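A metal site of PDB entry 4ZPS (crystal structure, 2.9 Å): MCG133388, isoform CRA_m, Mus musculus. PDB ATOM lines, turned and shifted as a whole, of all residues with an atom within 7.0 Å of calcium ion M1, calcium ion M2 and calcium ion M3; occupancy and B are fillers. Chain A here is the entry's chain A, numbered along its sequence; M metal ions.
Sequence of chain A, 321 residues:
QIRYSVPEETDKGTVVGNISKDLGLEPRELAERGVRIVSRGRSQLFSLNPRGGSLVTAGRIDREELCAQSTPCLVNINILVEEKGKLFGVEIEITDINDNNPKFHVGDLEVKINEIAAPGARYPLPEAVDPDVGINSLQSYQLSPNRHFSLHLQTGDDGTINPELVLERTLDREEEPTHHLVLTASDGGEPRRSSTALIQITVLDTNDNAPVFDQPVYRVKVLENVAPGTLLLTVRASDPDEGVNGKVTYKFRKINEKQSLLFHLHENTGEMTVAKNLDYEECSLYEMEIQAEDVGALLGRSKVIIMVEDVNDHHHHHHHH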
ATOM      1  N   ASN A 114       9.561  10.102  14.869  1.00  0.00           N
ATOM      2  CA  ASN A 114      10.189   9.439  13.734  1.00  0.00           C
ATOM      3  C   ASN A 114       9.427   9.709  12.447  1.00  0.00           C
ATOM      4  O   ASN A 114       8.220   9.914  12.466  1.00  0.00           O
ATOM      5  CB  ASN A 114      10.285   7.930  13.998  1.00  0.00           C
ATOM      6  CG  ASN A 114      11.215   7.220  13.033  1.00  0.00           C
ATOM      7  OD1 ASN A 114      11.250   7.515  11.841  1.00  0.00           O
ATOM      8  ND2 ASN A 114      11.993   6.282  13.556  1.00  0.00           N
ATOM      9  N   GLU A 115      10.146   9.709  11.320  1.00  0.00           N
ATOM     10  CA  GLU A 115       9.540   9.931  10.014  1.00  0.00           C
ATOM     11  C   GLU A 115       8.482   8.894   9.677  1.00  0.00           C
ATOM     12  O   GLU A 115       7.507   9.196   8.987  1.00  0.00           O
ATOM     13  CB  GLU A 115      10.605   9.908   8.914  1.00  0.00           C
ATOM     14  CG  GLU A 115      11.592  11.044   8.920  1.00  0.00           C
ATOM     15  CD  GLU A 115      12.598  10.890   7.818  1.00  0.00           C
ATOM     16  OE1 GLU A 115      12.992   9.743   7.529  1.00  0.00           O
ATOM     17  OE2 GLU A 115      12.999  11.917   7.224  1.00  0.00           O
ATOM     18  N   LEU A 171       6.154  13.512   8.285  1.00  0.00           N
ATOM     19  CA  LEU A 171       7.390  14.283   8.414  1.00  0.00           C
ATOM     20  C   LEU A 171       8.494  13.689   7.525  1.00  0.00           C
ATOM     21  O   LEU A 171       8.354  12.579   7.004  1.00  0.00           O
ATOM     22  CB  LEU A 171       7.854  14.327   9.874  1.00  0.00           C
ATOM     23  CG  LEU A 171       6.928  15.082  10.838  1.00  0.00           C
ATOM     24  CD1 LEU A 171       7.373  14.888  12.280  1.00  0.00           C
ATOM     25  CD2 LEU A 171       6.889  16.558  10.498  1.00  0.00           C
ATOM     26  N   ASP A 172       9.577  14.446   7.364  1.00  0.00           N
ATOM     27  CA  ASP A 172      10.707  14.013   6.549  1.00  0.00           C
ATOM     28  C   ASP A 172      11.951  14.818   6.906  1.00  0.00           C
ATOM     29  O   ASP A 172      12.103  15.961   6.472  1.00  0.00           O
ATOM     30  CB  ASP A 172      10.385  14.148   5.062  1.00  0.00           C
ATOM     31  CG  ASP A 172      11.520  13.666   4.169  1.00  0.00           C
ATOM     32  OD1 ASP A 172      12.305  12.800   4.609  1.00  0.00           O
ATOM     33  OD2 ASP A 172      11.613  14.156   3.023  1.00  0.00           O
ATOM     34  N   ARG A 173      12.856  14.229   7.695  1.00  0.00           N
ATOM     35  CA  ARG A 173      14.054  14.939   8.135  1.00  0.00           C
ATOM     36  C   ARG A 173      15.064  15.103   7.002  1.00  0.00           C
ATOM     37  O   ARG A 173      16.018  15.867   7.108  1.00  0.00           O
ATOM     38  CB  ARG A 173      14.708  14.239   9.328  1.00  0.00           C
ATOM     39  CG  ARG A 173      15.357  12.911   9.000  1.00  0.00           C
ATOM     40  CD  ARG A 173      16.590  12.663   9.860  1.00  0.00           C
ATOM     41  NE  ARG A 173      17.674  13.586   9.526  1.00  0.00           N
ATOM     42  CZ  ARG A 173      18.531  13.400   8.527  1.00  0.00           C
ATOM     43  NH1 ARG A 173      18.424  12.331   7.756  1.00  0.00           N
ATOM     44  NH2 ARG A 173      19.483  14.291   8.297  1.00  0.00           N
ATOM     45  N   GLU A 174      14.857  14.363   5.919  1.00  0.00           N
ATOM     46  CA  GLU A 174      15.693  14.528   4.732  1.00  0.00           C
ATOM     47  C   GLU A 174      15.402  15.877   4.083  1.00  0.00           C
ATOM     48  O   GLU A 174      16.208  16.391   3.302  1.00  0.00           O
ATOM     49  CB  GLU A 174      15.468  13.386   3.732  1.00  0.00           C
ATOM     50  CG  GLU A 174      16.276  12.134   4.040  1.00  0.00           C
ATOM     51  CD  GLU A 174      15.768  11.369   5.250  1.00  0.00           C
ATOM     52  OE1 GLU A 174      16.434  11.398   6.300  1.00  0.00           O
ATOM     53  OE2 GLU A 174      14.699  10.727   5.141  1.00  0.00           O
ATOM     54  N   GLU A 175      14.255  16.449   4.427  1.00  0.00           N
ATOM     55  CA  GLU A 175      13.889  17.793   3.984  1.00  0.00           C
ATOM     56  C   GLU A 175      14.016  18.802   5.122  1.00  0.00           C
ATOM     57  O   GLU A 175      14.634  19.857   4.963  1.00  0.00           O
ATOM     58  CB  GLU A 175      12.457  17.810   3.425  1.00  0.00           C
ATOM     59  CG  GLU A 175      12.337  17.283   2.012  1.00  0.00           C
ATOM     60  CD  GLU A 175      12.930  18.237   0.978  1.00  0.00           C
ATOM     61  OE1 GLU A 175      13.173  19.410   1.324  1.00  0.00           O
ATOM     62  OE2 GLU A 175      13.137  17.810  -0.172  1.00  0.00           O
ATOM     63  N   LEU A 204      13.282  12.329  14.237  1.00  0.00           N
ATOM     64  CA  LEU A 204      14.246  11.240  14.246  1.00  0.00           C
ATOM     65  C   LEU A 204      14.289  10.576  12.876  1.00  0.00           C
ATOM     66  O   LEU A 204      13.361  10.712  12.084  1.00  0.00           O
ATOM     67  CB  LEU A 204      13.912  10.219  15.328  1.00  0.00           C
ATOM     68  CG  LEU A 204      13.780  10.787  16.740  1.00  0.00           C
ATOM     69  CD1 LEU A 204      13.590   9.673  17.769  1.00  0.00           C
ATOM     70  CD2 LEU A 204      14.976  11.647  17.099  1.00  0.00           C
ATOM     71  N   ASP A 205      15.376   9.862  12.594  1.00  0.00           N
ATOM     72  CA  ASP A 205      15.579   9.292  11.268  1.00  0.00           C
ATOM     73  C   ASP A 205      15.093   7.857  11.149  1.00  0.00           C
ATOM     74  O   ASP A 205      15.123   7.094  12.123  1.00  0.00           O
ATOM     75  CB  ASP A 205      17.066   9.350  10.896  1.00  0.00           C
ATOM     76  CG  ASP A 205      17.324   8.937   9.453  1.00  0.00           C
ATOM     77  OD1 ASP A 205      17.225   9.791   8.547  1.00  0.00           O
ATOM     78  OD2 ASP A 205      17.638   7.745   9.221  1.00  0.00           O
ATOM     79  N   THR A 206      14.634   7.505   9.959  1.00  0.00           N
ATOM     80  CA  THR A 206      14.389   6.109   9.591  1.00  0.00           C
ATOM     81  C   THR A 206      15.082   5.852   8.256  1.00  0.00           C
ATOM     82  O   THR A 206      15.272   6.765   7.460  1.00  0.00           O
ATOM     83  CB  THR A 206      12.884   5.795   9.483  1.00  0.00           C
ATOM     84  OG1 THR A 206      12.715   4.401   9.160  1.00  0.00           O
ATOM     85  CG2 THR A 206      12.229   6.642   8.402  1.00  0.00           C
ATOM     86  N   ASN A 207      15.490   4.611   8.035  1.00  0.00           N
ATOM     87  CA  ASN A 207      16.237   4.260   6.824  1.00  0.00           C
ATOM     88  C   ASN A 207      15.297   3.959   5.653  1.00  0.00           C
ATOM     89  O   ASN A 207      15.025   2.797   5.348  1.00  0.00           O
ATOM     90  CB  ASN A 207      17.151   3.066   7.093  1.00  0.00           C
ATOM     91  CG  ASN A 207      18.022   2.726   5.910  1.00  0.00           C
ATOM     92  OD1 ASN A 207      19.006   3.403   5.628  1.00  0.00           O
ATOM     93  ND2 ASN A 207      17.669   1.657   5.207  1.00  0.00           N
ATOM     94  N   ASP A 208      14.814   5.010   5.003  1.00  0.00           N
ATOM     95  CA  ASP A 208      13.859   4.859   3.914  1.00  0.00           C
ATOM     96  C   ASP A 208      14.461   5.242   2.565  1.00  0.00           C
ATOM     97  O   ASP A 208      13.886   4.950   1.513  1.00  0.00           O
ATOM     98  CB  ASP A 208      12.607   5.694   4.187  1.00  0.00           C
ATOM     99  CG  ASP A 208      12.913   7.145   4.504  1.00  0.00           C
ATOM    100  OD1 ASP A 208      13.998   7.424   5.064  1.00  0.00           O
ATOM    101  OD2 ASP A 208      12.080   8.018   4.188  1.00  0.00           O
ATOM    102  N   ASN A 209      15.614   5.894   2.592  1.00  0.00           N
ATOM    103  CA  ASN A 209      16.322   6.223   1.354  1.00  0.00           C
ATOM    104  C   ASN A 209      17.340   5.165   0.964  1.00  0.00           C
ATOM    105  O   ASN A 209      18.346   4.976   1.650  1.00  0.00           O
ATOM    106  CB  ASN A 209      17.008   7.589   1.479  1.00  0.00           C
ATOM    107  CG  ASN A 209      16.034   8.737   1.391  1.00  0.00           C
ATOM    108  OD1 ASN A 209      15.752   9.395   2.397  1.00  0.00           O
ATOM    109  ND2 ASN A 209      15.517   8.999   0.200  1.00  0.00           N
ATOM    110  N   ALA A 210      17.069   4.468  -0.128  1.00  0.00           N
ATOM    111  CA  ALA A 210      17.996   3.485  -0.669  1.00  0.00           C
ATOM    112  C   ALA A 210      19.073   4.181  -1.484  1.00  0.00           C
ATOM    113  O   ALA A 210      18.829   5.226  -2.087  1.00  0.00           O
ATOM    114  CB  ALA A 210      17.257   2.464  -1.523  1.00  0.00           C
ATOM    115  N   PRO A 211      20.293   3.618  -1.496  1.00  0.00           N
ATOM    116  CA  PRO A 211      21.403   4.145  -2.293  1.00  0.00           C
ATOM    117  C   PRO A 211      21.070   4.275  -3.774  1.00  0.00           C
ATOM    118  O   PRO A 211      20.530   3.340  -4.366  1.00  0.00           O
ATOM    119  CB  PRO A 211      22.515   3.112  -2.075  1.00  0.00           C
ATOM    120  CG  PRO A 211      22.208   2.520  -0.742  1.00  0.00           C
ATOM    121  CD  PRO A 211      20.706   2.479  -0.657  1.00  0.00           C
ATOM    122  N   SER A 238      24.008   8.414  -3.861  1.00  0.00           N
ATOM    123  CA  SER A 238      23.377   9.349  -2.936  1.00  0.00           C
ATOM    124  C   SER A 238      22.535   8.623  -1.877  1.00  0.00           C
ATOM    125  O   SER A 238      21.837   7.661  -2.174  1.00  0.00           O
ATOM    126  CB  SER A 238      22.501  10.336  -3.693  1.00  0.00           C
ATOM    127  OG  SER A 238      21.875  11.252  -2.812  1.00  0.00           O
ATOM    128  N   ASP A 239      22.618   9.112  -0.646  1.00  0.00           N
ATOM    129  CA  ASP A 239      21.840   8.576   0.465  1.00  0.00           C
ATOM    130  C   ASP A 239      21.709   9.628   1.552  1.00  0.00           C
ATOM    131  O   ASP A 239      22.610   9.778   2.384  1.00  0.00           O
ATOM    132  CB  ASP A 239      22.494   7.303   1.012  1.00  0.00           C
ATOM    133  CG  ASP A 239      21.519   6.423   1.756  1.00  0.00           C
ATOM    134  OD1 ASP A 239      20.595   6.961   2.407  1.00  0.00           O
ATOM    135  OD2 ASP A 239      21.670   5.182   1.694  1.00  0.00           O
ATOM    136  N   PRO A 240      20.594  10.365   1.561  1.00  0.00           N
ATOM    137  CA  PRO A 240      20.372  11.516   2.443  1.00  0.00           C
ATOM    138  C   PRO A 240      20.069  11.129   3.881  1.00  0.00           C
ATOM    139  O   PRO A 240      19.936  12.011   4.731  1.00  0.00           O
ATOM    140  CB  PRO A 240      19.155  12.214   1.813  1.00  0.00           C
ATOM    141  CG  PRO A 240      18.938  11.554   0.481  1.00  0.00           C
ATOM    142  CD  PRO A 240      19.467  10.175   0.628  1.00  0.00           C
ATOM    143  N   ASP A 241      19.952   9.826   4.155  1.00  0.00           N
ATOM    144  CA  ASP A 241      19.656   9.355   5.505  1.00  0.00           C
ATOM    145  C   ASP A 241      20.752   9.760   6.490  1.00  0.00           C
ATOM    146  O   ASP A 241      21.859  10.102   6.093  1.00  0.00           O
ATOM    147  CB  ASP A 241      19.467   7.838   5.508  1.00  0.00           C
ATOM    148  CG  ASP A 241      18.231   7.407   4.747  1.00  0.00           C
ATOM    149  OD1 ASP A 241      17.311   8.232   4.589  1.00  0.00           O
ATOM    150  OD2 ASP A 241      18.182   6.234   4.314  1.00  0.00           O
ATOM    151  N   GLU A 242      20.424   9.707   7.774  1.00  0.00           N
ATOM    152  CA  GLU A 242      21.307  10.227   8.809  1.00  0.00           C
ATOM    153  C   GLU A 242      22.371   9.219   9.247  1.00  0.00           C
ATOM    154  O   GLU A 242      22.059   8.071   9.556  1.00  0.00           O
ATOM    155  CB  GLU A 242      20.499  10.678  10.020  1.00  0.00           C
ATOM    156  CG  GLU A 242      21.328  11.327  11.122  1.00  0.00           C
ATOM    157  CD  GLU A 242      20.452  11.929  12.216  1.00  0.00           C
ATOM    158  OE1 GLU A 242      19.221  11.729  12.166  1.00  0.00           O
ATOM    159  OE2 GLU A 242      21.007  12.602  13.113  1.00  0.00           O
ATOM    160  N   VAL A 244      24.665   6.494  10.051  1.00  0.00           N
ATOM    161  CA  VAL A 244      24.867   5.098   9.695  1.00  0.00           C
ATOM    162  C   VAL A 244      23.972   4.684   8.529  1.00  0.00           C
ATOM    163  O   VAL A 244      24.370   3.899   7.662  1.00  0.00           O
ATOM    164  CB  VAL A 244      24.603   4.177  10.905  1.00  0.00           C
ATOM    165  CG1 VAL A 244      25.072   2.768  10.598  1.00  0.00           C
ATOM    166  CG2 VAL A 244      25.306   4.713  12.137  1.00  0.00           C
ATOM    167  N   ASN A 245      22.752   5.220   8.495  1.00  0.00           N
ATOM    168  CA  ASN A 245      21.812   4.935   7.434  1.00  0.00           C
ATOM    169  C   ASN A 245      22.201   5.617   6.114  1.00  0.00           C
ATOM    170  O   ASN A 245      21.613   5.343   5.070  1.00  0.00           O
ATOM    171  CB  ASN A 245      20.403   5.363   7.832  1.00  0.00           C
ATOM    172  CG  ASN A 245      19.868   4.596   9.018  1.00  0.00           C
ATOM    173  OD1 ASN A 245      20.079   3.389   9.146  1.00  0.00           O
ATOM    174  ND2 ASN A 245      19.168   5.293   9.906  1.00  0.00           N
ATOM    175  N   GLY A 246      23.190   6.497   6.188  1.00  0.00           N
ATOM    176  CA  GLY A 246      23.638   7.222   5.009  1.00  0.00           C
ATOM    177  C   GLY A 246      24.998   6.755   4.536  1.00  0.00           C
ATOM    178  O   GLY A 246      25.483   7.190   3.489  1.00  0.00           O
ATOM    179  N   LYS A 247      25.619   5.869   5.307  1.00  0.00           N
ATOM    180  CA  LYS A 247      26.902   5.299   4.935  1.00  0.00           C
ATOM    181  C   LYS A 247      26.743   4.356   3.752  1.00  0.00           C
ATOM    182  O   LYS A 247      26.090   3.323   3.853  1.00  0.00           O
ATOM    183  CB  LYS A 247      27.536   4.567   6.107  1.00  0.00           C
ATOM    184  CG  LYS A 247      28.894   3.959   5.810  1.00  0.00           C
ATOM    185  CD  LYS A 247      29.476   3.253   7.023  1.00  0.00           C
ATOM    186  CE  LYS A 247      30.785   2.554   6.673  1.00  0.00           C
ATOM    187  NZ  LYS A 247      31.382   1.869   7.847  1.00  0.00           N
ATOM    188  N   ASP A 294      23.755   0.154   1.855  1.00  0.00           N
ATOM    189  CA  ASP A 294      23.753   0.775   3.180  1.00  0.00           C
ATOM    190  C   ASP A 294      23.509  -0.289   4.252  1.00  0.00           C
ATOM    191  O   ASP A 294      23.285  -1.456   3.937  1.00  0.00           O
ATOM    192  CB  ASP A 294      22.702   1.877   3.272  1.00  0.00           C
ATOM    193  CG  ASP A 294      21.284   1.347   3.182  1.00  0.00           C
ATOM    194  OD1 ASP A 294      21.096   0.217   2.682  1.00  0.00           O
ATOM    195  OD2 ASP A 294      20.356   2.065   3.604  1.00  0.00           O
ATOM    196  N   VAL A 295      23.533   0.123   5.518  1.00  0.00           N
ATOM    197  CA  VAL A 295      23.404  -0.816   6.618  1.00  0.00           C
ATOM    198  C   VAL A 295      22.032  -1.476   6.675  1.00  0.00           C
ATOM    199  O   VAL A 295      21.859  -2.514   7.321  1.00  0.00           O
ATOM    200  CB  VAL A 295      23.681  -0.125   7.968  1.00  0.00           C
ATOM    201  CG1 VAL A 295      25.139   0.295   8.056  1.00  0.00           C
ATOM    202  CG2 VAL A 295      22.756   1.069   8.157  1.00  0.00           C
ATOM    203  N   GLY A 296      21.057  -0.875   6.001  1.00  0.00           N
ATOM    204  CA  GLY A 296      19.729  -1.445   5.945  1.00  0.00           C
ATOM    205  C   GLY A 296      19.584  -2.457   4.820  1.00  0.00           C
ATOM    206  O   GLY A 296      18.483  -2.909   4.523  1.00  0.00           O
ATOM    207  N   LEU A 298      19.846  -1.991   1.695  1.00  0.00           N
ATOM    208  CA  LEU A 298      19.165  -1.448   0.530  1.00  0.00           C
ATOM    209  C   LEU A 298      20.163  -1.264  -0.608  1.00  0.00           C
ATOM    210  O   LEU A 298      21.256  -0.739  -0.411  1.00  0.00           O
ATOM    211  CB  LEU A 298      18.482  -0.121   0.854  1.00  0.00           C
ATOM    212  CG  LEU A 298      17.449  -0.112   1.978  1.00  0.00           C
ATOM    213  CD1 LEU A 298      16.781   1.254   2.051  1.00  0.00           C
ATOM    214  CD2 LEU A 298      16.410  -1.205   1.800  1.00  0.00           C
HETATM  215 CA    CA M   1      19.928   4.626   3.423  1.00  0.00          CA
HETATM  216 CA    CA M   2      15.685   9.123   6.728  1.00  0.00          CA
HETATM  217 CA    CA M   3      12.251  10.426   4.676  1.00  0.00          CA
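Calcium ion M1 is bound by O of Asn 209 (2.4 Å), O of Asn 245 (2.5 Å), OD2 of Asp 239 (2.5 Å), OD2 of Asp 241 (2.5 Å), OD2 of Asp 294 (2.6 Å), OD1 of Asp 239 (2.6 Å) and OD1 of Asn 207 (2.7 Å).
Calcium ion M1 has seven donor atoms within binding distance.
Calcium ion M2 is bound by OE1 of Glu 174 (2.4 Å).
The side-chain carboxylate (OE2) of Glu 174 is bound to calcium ion M2, 2.5 Å away.
Calcium ion M2 is bound by OD1 of Asp 205 (2.5 Å).
The backbone carbonyl oxygen (O) of Thr 206 is bound to calcium ion M2, at 2.5 Å.
Calcium ion M2 is bound by OD1 of Asp 241, at 2.8 Å.
OE1 of Glu 115 binds calcium ion M2 (2.9 Å).
Slightly farther from calcium ion M2 lies the side-chain carboxylate (OD1) of Asp 208 (2.9 Å).
Within 4 Å of calcium ion M2: Glu 115, Glu 174, Asp 205, Thr 206, Asp 208 and Asp 241.
The nearest printed residue that does not touch calcium ion M2 is Asn 209 (4.3 Å).
OD1 of Asp 172 binds calcium ion M3, 2.4 Å away.
Calcium ion M3 is bound by the side-chain carboxylate (OD2) of Asp 208.
OE2 of Glu 174 binds calcium ion M3, at 2.5 Å.
Slightly farther from calcium ion M3 lies the side-chain carboxylate (OE1) of Glu 115 (3.0 Å).
Slightly farther from calcium ion M3 lies OE2 of Glu 115 (3.0 Å).
The side-chain carboxylate (OD1) of Asp 294 sits at hydrogen-bond distance from the backbone NH (N) of Leu 298, 2.7 Å away.
The backbone carbonyl oxygen of Leu 204 is in hydrogen-bond range of the backbone NH of Glu 115 (3.5 Å).
The side-chain carboxylate of Asp 205 sits at hydrogen-bond distance from the side-chain amide nitrogen of Asn 245, at 3.0 Å.
NH1 of Arg 173 lies close to OD1 of Asp 205 (2.9 Å).
OD1 of Asp 294 sits close to N of Gly 296, 3.5 Å away.
OD1 of Asn 209 sits close to OE2 of Glu 174 (3.2 Å).
The backbone NH (N) of Glu 242 lies close to the side-chain carboxylate (OD1) of Asp 205, 3.3 Å away.
OE1 of Glu 174 sits close to NH1 of Arg 173.
Within 4 Å of calcium ion M1: Asn 207, Asn 209, Asp 239, Asp 241, Asn 245 and Asp 294.
The nearest printed residue that does not touch calcium ion M1 is Ala 210 (4.6 Å).
Four residues have an atom within 4 Å of calcium ion M3: Glu 115, Asp 172, Glu 174 and Asp 208.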
